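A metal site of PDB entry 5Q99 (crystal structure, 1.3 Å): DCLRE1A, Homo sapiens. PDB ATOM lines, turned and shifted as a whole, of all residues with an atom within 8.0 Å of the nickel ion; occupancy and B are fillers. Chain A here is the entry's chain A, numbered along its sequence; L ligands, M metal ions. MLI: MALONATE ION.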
ATOM      1  N   ASP A  18      -3.230  17.231 -10.721  1.00  0.00           N
ATOM      2  CA  ASP A  18      -2.256  16.893 -11.773  1.00  0.00           C
ATOM      3  C   ASP A  18      -1.342  15.644 -11.406  1.00  0.00           C
ATOM      4  O   ASP A  18      -0.104  15.656 -11.675  1.00  0.00           O
ATOM      5  CB  ASP A  18      -1.462  18.109 -12.186  1.00  0.00           C
ATOM      6  CG  ASP A  18      -2.355  19.284 -12.669  1.00  0.00           C
ATOM      7  OD1 ASP A  18      -3.566  19.052 -13.012  1.00  0.00           O
ATOM      8  OD2 ASP A  18      -1.750  20.400 -12.802  1.00  0.00           O
ATOM      9  N   THR A  34      -5.679  20.562 -13.930  1.00  0.00           N
ATOM     10  CA  THR A  34      -5.720  22.008 -14.178  1.00  0.00           C
ATOM     11  C   THR A  34      -5.760  22.430 -15.667  1.00  0.00           C
ATOM     12  O   THR A  34      -6.403  23.425 -15.982  1.00  0.00           O
ATOM     13  CB  THR A  34      -4.574  22.745 -13.436  1.00  0.00           C
ATOM     14  OG1 THR A  34      -3.304  22.330 -14.009  1.00  0.00           O
ATOM     15  CG2 THR A  34      -4.608  22.513 -11.919  1.00  0.00           C
ATOM     16  N   HIS A  35      -5.127  21.632 -16.525  1.00  0.00           N
ATOM     17  CA  HIS A  35      -5.036  21.970 -17.943  1.00  0.00           C
ATOM     18  C   HIS A  35      -4.461  20.800 -18.701  1.00  0.00           C
ATOM     19  O   HIS A  35      -3.792  19.893 -18.146  1.00  0.00           O
ATOM     20  CB  HIS A  35      -4.179  23.282 -18.200  1.00  0.00           C
ATOM     21  CG  HIS A  35      -2.730  23.217 -17.852  1.00  0.00           C
ATOM     22  ND1 HIS A  35      -2.184  23.081 -16.590  1.00  0.00           N
ATOM     23  CD2 HIS A  35      -1.662  23.331 -18.687  1.00  0.00           C
ATOM     24  CE1 HIS A  35      -0.855  23.106 -16.686  1.00  0.00           C
ATOM     25  NE2 HIS A  35      -0.528  23.291 -17.942  1.00  0.00           N
ATOM     26  N   PHE A  36      -4.736  20.890 -20.021  1.00  0.00           N
ATOM     27  CA  PHE A  36      -4.297  19.817 -20.962  1.00  0.00           C
ATOM     28  C   PHE A  36      -2.881  20.003 -21.494  1.00  0.00           C
ATOM     29  O   PHE A  36      -2.695  20.247 -22.758  1.00  0.00           O
ATOM     30  CB  PHE A  36      -5.371  19.690 -22.103  1.00  0.00           C
ATOM     31  CG  PHE A  36      -5.275  18.377 -22.938  1.00  0.00           C
ATOM     32  CD1 PHE A  36      -5.719  17.170 -22.416  1.00  0.00           C
ATOM     33  CD2 PHE A  36      -4.711  18.414 -24.224  1.00  0.00           C
ATOM     34  CE1 PHE A  36      -5.616  15.998 -23.166  1.00  0.00           C
ATOM     35  CE2 PHE A  36      -4.641  17.225 -24.968  1.00  0.00           C
ATOM     36  CZ  PHE A  36      -5.084  16.059 -24.444  1.00  0.00           C
ATOM     37  N   HIS A  37      -1.838  19.916 -20.647  1.00  0.00           N
ATOM     38  CA  HIS A  37      -0.424  19.822 -21.023  1.00  0.00           C
ATOM     39  C   HIS A  37       0.128  18.452 -20.531  1.00  0.00           C
ATOM     40  O   HIS A  37      -0.222  18.002 -19.423  1.00  0.00           O
ATOM     41  CB  HIS A  37       0.465  20.996 -20.494  1.00  0.00           C
ATOM     42  CG  HIS A  37       0.351  22.263 -21.298  1.00  0.00           C
ATOM     43  ND1 HIS A  37       0.739  23.503 -20.835  1.00  0.00           N
ATOM     44  CD2 HIS A  37      -0.134  22.468 -22.548  1.00  0.00           C
ATOM     45  CE1 HIS A  37       0.561  24.413 -21.772  1.00  0.00           C
ATOM     46  NE2 HIS A  37       0.051  23.798 -22.837  1.00  0.00           N
ATOM     47  N   SER A  38       1.000  17.822 -21.367  1.00  0.00           N
ATOM     48  CA  SER A  38       1.344  16.385 -21.139  1.00  0.00           C
ATOM     49  C   SER A  38       2.081  16.152 -19.798  1.00  0.00           C
ATOM     50  O   SER A  38       1.802  15.109 -19.121  1.00  0.00           O
ATOM     51  CB  SER A  38       2.079  15.828 -22.343  1.00  0.00           C
ATOM     52  OG  SER A  38       3.265  16.542 -22.515  1.00  0.00           O
ATOM     53  N   ASP A  39       2.852  17.092 -19.290  1.00  0.00           N
ATOM     54  CA  ASP A  39       3.467  16.855 -17.961  1.00  0.00           C
ATOM     55  C   ASP A  39       2.461  16.847 -16.842  1.00  0.00           C
ATOM     56  O   ASP A  39       2.748  16.336 -15.719  1.00  0.00           O
ATOM     57  CB  ASP A  39       4.507  17.873 -17.640  1.00  0.00           C
ATOM     58  CG  ASP A  39       5.913  17.614 -18.315  1.00  0.00           C
ATOM     59  OD1 ASP A  39       6.108  16.553 -18.964  1.00  0.00           O
ATOM     60  OD2 ASP A  39       6.767  18.519 -18.231  1.00  0.00           O
ATOM     61  N   HIS A  40       1.245  17.373 -17.083  1.00  0.00           N
ATOM     62  CA  HIS A  40       0.133  17.324 -16.111  1.00  0.00           C
ATOM     63  C   HIS A  40      -0.829  16.212 -16.307  1.00  0.00           C
ATOM     64  O   HIS A  40      -1.310  15.670 -15.285  1.00  0.00           O
ATOM     65  CB  HIS A  40      -0.521  18.767 -16.149  1.00  0.00           C
ATOM     66  CG  HIS A  40       0.428  19.850 -15.792  1.00  0.00           C
ATOM     67  ND1 HIS A  40       0.450  20.497 -14.570  1.00  0.00           N
ATOM     68  CD2 HIS A  40       1.397  20.456 -16.507  1.00  0.00           C
ATOM     69  CE1 HIS A  40       1.428  21.355 -14.514  1.00  0.00           C
ATOM     70  NE2 HIS A  40       2.030  21.343 -15.687  1.00  0.00           N
ATOM     71  N   HIS A  96      -3.385  30.988 -18.820  1.00  0.00           N
ATOM     72  CA  HIS A  96      -2.322  30.064 -19.326  1.00  0.00           C
ATOM     73  C   HIS A  96      -2.720  29.699 -20.722  1.00  0.00           C
ATOM     74  O   HIS A  96      -2.809  30.662 -21.576  1.00  0.00           O
ATOM     75  CB  HIS A  96      -2.037  28.910 -18.327  1.00  0.00           C
ATOM     76  CG  HIS A  96      -0.932  27.981 -18.682  1.00  0.00           C
ATOM     77  ND1 HIS A  96       0.357  28.382 -18.910  1.00  0.00           N
ATOM     78  CD2 HIS A  96      -0.928  26.631 -18.750  1.00  0.00           C
ATOM     79  CE1 HIS A  96       1.097  27.286 -19.163  1.00  0.00           C
ATOM     80  NE2 HIS A  96       0.364  26.202 -19.033  1.00  0.00           N
ATOM     81  N   CYS A  97      -2.952  28.436 -21.032  1.00  0.00           N
ATOM     82  CA  CYS A  97      -3.493  27.934 -22.319  1.00  0.00           C
ATOM     83  C   CYS A  97      -5.032  27.837 -22.268  1.00  0.00           C
ATOM     84  O   CYS A  97      -5.628  27.870 -21.178  1.00  0.00           O
ATOM     85  CB  CYS A  97      -2.806  26.614 -22.684  1.00  0.00           C
ATOM     86  SG  CYS A  97      -3.217  25.257 -21.503  1.00  0.00           S
ATOM     87  N   ALA A 100      -7.312  26.304 -19.129  1.00  0.00           N
ATOM     88  CA  ALA A 100      -6.478  26.205 -17.920  1.00  0.00           C
ATOM     89  C   ALA A 100      -7.107  26.986 -16.773  1.00  0.00           C
ATOM     90  O   ALA A 100      -7.553  28.134 -16.948  1.00  0.00           O
ATOM     91  CB  ALA A 100      -5.065  26.722 -18.138  1.00  0.00           C
ATOM     92  N   GLY A 117      -2.362  25.944 -10.516  1.00  0.00           N
ATOM     93  CA  GLY A 117      -1.906  25.152 -11.676  1.00  0.00           C
ATOM     94  C   GLY A 117      -0.765  25.851 -12.346  1.00  0.00           C
ATOM     95  O   GLY A 117       0.085  26.368 -11.652  1.00  0.00           O
ATOM     96  N   ASP A 118      -0.741  25.891 -13.689  1.00  0.00           N
ATOM     97  CA  ASP A 118       0.189  26.791 -14.433  1.00  0.00           C
ATOM     98  C   ASP A 118      -0.609  28.104 -14.687  1.00  0.00           C
ATOM     99  O   ASP A 118      -1.770  28.043 -15.098  1.00  0.00           O
ATOM    100  CB  ASP A 118       0.673  26.221 -15.758  1.00  0.00           C
ATOM    101  CG  ASP A 118       1.742  25.151 -15.668  1.00  0.00           C
ATOM    102  OD1 ASP A 118       2.360  24.964 -14.612  1.00  0.00           O
ATOM    103  OD2 ASP A 118       2.054  24.537 -16.731  1.00  0.00           O
ATOM    104  N   PHE A 119       0.032  29.259 -14.477  1.00  0.00           N
ATOM    105  CA  PHE A 119      -0.663  30.572 -14.678  1.00  0.00           C
ATOM    106  C   PHE A 119       0.291  31.652 -15.143  1.00  0.00           C
ATOM    107  O   PHE A 119       1.486  31.584 -14.879  1.00  0.00           O
ATOM    108  CB  PHE A 119      -1.512  30.993 -13.371  1.00  0.00           C
ATOM    109  CG  PHE A 119      -0.805  31.736 -12.273  1.00  0.00           C
ATOM    110  CD1 PHE A 119      -1.428  32.767 -11.601  1.00  0.00           C
ATOM    111  CD2 PHE A 119       0.477  31.363 -11.816  1.00  0.00           C
ATOM    112  CE1 PHE A 119      -0.852  33.416 -10.561  1.00  0.00           C
ATOM    113  CE2 PHE A 119       1.117  32.043 -10.731  1.00  0.00           C
ATOM    114  CZ  PHE A 119       0.435  33.047 -10.097  1.00  0.00           C
ATOM    115  N   ASP A 141       2.758  28.200  -9.106  1.00  0.00           N
ATOM    116  CA  ASP A 141       3.570  27.975 -10.320  1.00  0.00           C
ATOM    117  C   ASP A 141       4.794  28.925 -10.295  1.00  0.00           C
ATOM    118  O   ASP A 141       4.662  30.150 -10.591  1.00  0.00           O
ATOM    119  CB  ASP A 141       2.730  28.220 -11.585  1.00  0.00           C
ATOM    120  CG  ASP A 141       3.539  28.308 -12.889  1.00  0.00           C
ATOM    121  OD1 ASP A 141       4.737  27.893 -12.862  1.00  0.00           O
ATOM    122  OD2 ASP A 141       2.940  28.772 -13.910  1.00  0.00           O
ATOM    123  N   THR A 143       7.628  28.619 -12.164  1.00  0.00           N
ATOM    124  CA  THR A 143       8.433  28.360 -13.366  1.00  0.00           C
ATOM    125  C   THR A 143       9.527  29.371 -13.533  1.00  0.00           C
ATOM    126  O   THR A 143      10.714  28.965 -13.732  1.00  0.00           O
ATOM    127  CB  THR A 143       7.509  28.280 -14.635  1.00  0.00           C
ATOM    128  OG1 THR A 143       6.630  27.170 -14.552  1.00  0.00           O
ATOM    129  CG2 THR A 143       8.385  28.116 -15.901  1.00  0.00           C
ATOM    130  N   SER A 183       1.913  21.827 -28.500  1.00  0.00           N
ATOM    131  CA  SER A 183       0.892  21.589 -27.528  1.00  0.00           C
ATOM    132  C   SER A 183      -0.168  22.711 -27.721  1.00  0.00           C
ATOM    133  O   SER A 183       0.100  23.677 -28.466  1.00  0.00           O
ATOM    134  CB  SER A 183       1.499  21.822 -26.125  1.00  0.00           C
ATOM    135  OG  SER A 183       2.177  23.096 -26.092  1.00  0.00           O
ATOM    136  N   ILE A 184      -1.287  22.662 -27.039  1.00  0.00           N
ATOM    137  CA  ILE A 184      -2.160  23.804 -27.007  1.00  0.00           C
ATOM    138  C   ILE A 184      -1.535  24.985 -26.264  1.00  0.00           C
ATOM    139  O   ILE A 184      -0.562  24.793 -25.482  1.00  0.00           O
ATOM    140  CB  ILE A 184      -3.538  23.472 -26.318  1.00  0.00           C
ATOM    141  CG1 ILE A 184      -3.457  23.128 -24.796  1.00  0.00           C
ATOM    142  CG2 ILE A 184      -4.269  22.356 -27.095  1.00  0.00           C
ATOM    143  CD1 ILE A 184      -4.805  23.099 -24.134  1.00  0.00           C
ATOM    144  N   GLU A 296       3.256  32.109 -21.546  1.00  0.00           N
ATOM    145  CA  GLU A 296       2.013  31.848 -20.829  1.00  0.00           C
ATOM    146  C   GLU A 296       2.244  31.482 -19.354  1.00  0.00           C
ATOM    147  O   GLU A 296       1.388  30.912 -18.669  1.00  0.00           O
ATOM    148  CB  GLU A 296       1.150  30.827 -21.549  1.00  0.00           C
ATOM    149  CG  GLU A 296       0.558  31.333 -22.921  1.00  0.00           C
ATOM    150  CD  GLU A 296      -0.389  30.412 -23.645  1.00  0.00           C
ATOM    151  OE1 GLU A 296      -0.425  29.195 -23.388  1.00  0.00           O
ATOM    152  OE2 GLU A 296      -1.147  30.943 -24.518  1.00  0.00           O
ATOM    153  N   HIS A 297       3.433  31.867 -18.820  1.00  0.00           N
ATOM    154  CA  HIS A 297       3.747  31.852 -17.395  1.00  0.00           C
ATOM    155  C   HIS A 297       4.099  33.249 -16.841  1.00  0.00           C
ATOM    156  O   HIS A 297       4.635  34.096 -17.626  1.00  0.00           O
ATOM    157  CB  HIS A 297       4.971  30.894 -17.033  1.00  0.00           C
ATOM    158  CG  HIS A 297       4.744  29.416 -17.326  1.00  0.00           C
ATOM    159  ND1 HIS A 297       4.145  28.535 -16.452  1.00  0.00           N
ATOM    160  CD2 HIS A 297       5.099  28.665 -18.416  1.00  0.00           C
ATOM    161  CE1 HIS A 297       4.177  27.304 -16.959  1.00  0.00           C
ATOM    162  NE2 HIS A 297       4.702  27.398 -18.157  1.00  0.00           N
HETATM  163  C1  MLI L   1       4.215  23.122 -20.240  1.00  0.00           C
HETATM  164  C2  MLI L   1       4.204  24.621 -19.868  1.00  0.00           C
HETATM  165  C3  MLI L   1       3.695  22.267 -19.072  1.00  0.00           C
HETATM  166  O6  MLI L   1       5.262  25.295 -19.890  1.00  0.00           O
HETATM  167  O7  MLI L   1       3.114  25.087 -19.514  1.00  0.00           O
HETATM  168  O8  MLI L   1       2.600  22.478 -18.575  1.00  0.00           O
HETATM  169  O9  MLI L   1       4.341  21.257 -18.616  1.00  0.00           O
HETATM  170 NI    NI M   1       1.373  24.155 -18.788  1.00  0.00          NI
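The side-chain carboxylate (OD2) of Asp 118 lies close to a ring nitrogen (NE2) of His 40, 3.4 Å away. A ring nitrogen (NE2) of His 37 is in hydrogen-bond range of the backbone carbonyl oxygen (O) of Ile 184, 2.9 Å away. A ring nitrogen (ND1) of His 35 lies within hydrogen-bond range of the side-chain hydroxyl (OG1) of Thr 34, 2.9 Å away. The backbone carbonyl oxygen of Glu 296 sits at hydrogen-bond distance from a ring nitrogen (ND1) of His 96 (2.7 Å).
The nearest printed residue that does not touch the nickel ion is His 40 (4.2 Å).
The nickel ion is bound by O8 of the ligand (2.1 Å), O7 of the ligand (2.1 Å), OD2 of Asp 118 (2.2 Å), ND1 of His 37 (2.2 Å), NE2 of His 35 (2.3 Å) and NE2 of His 96 (2.3 Å).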
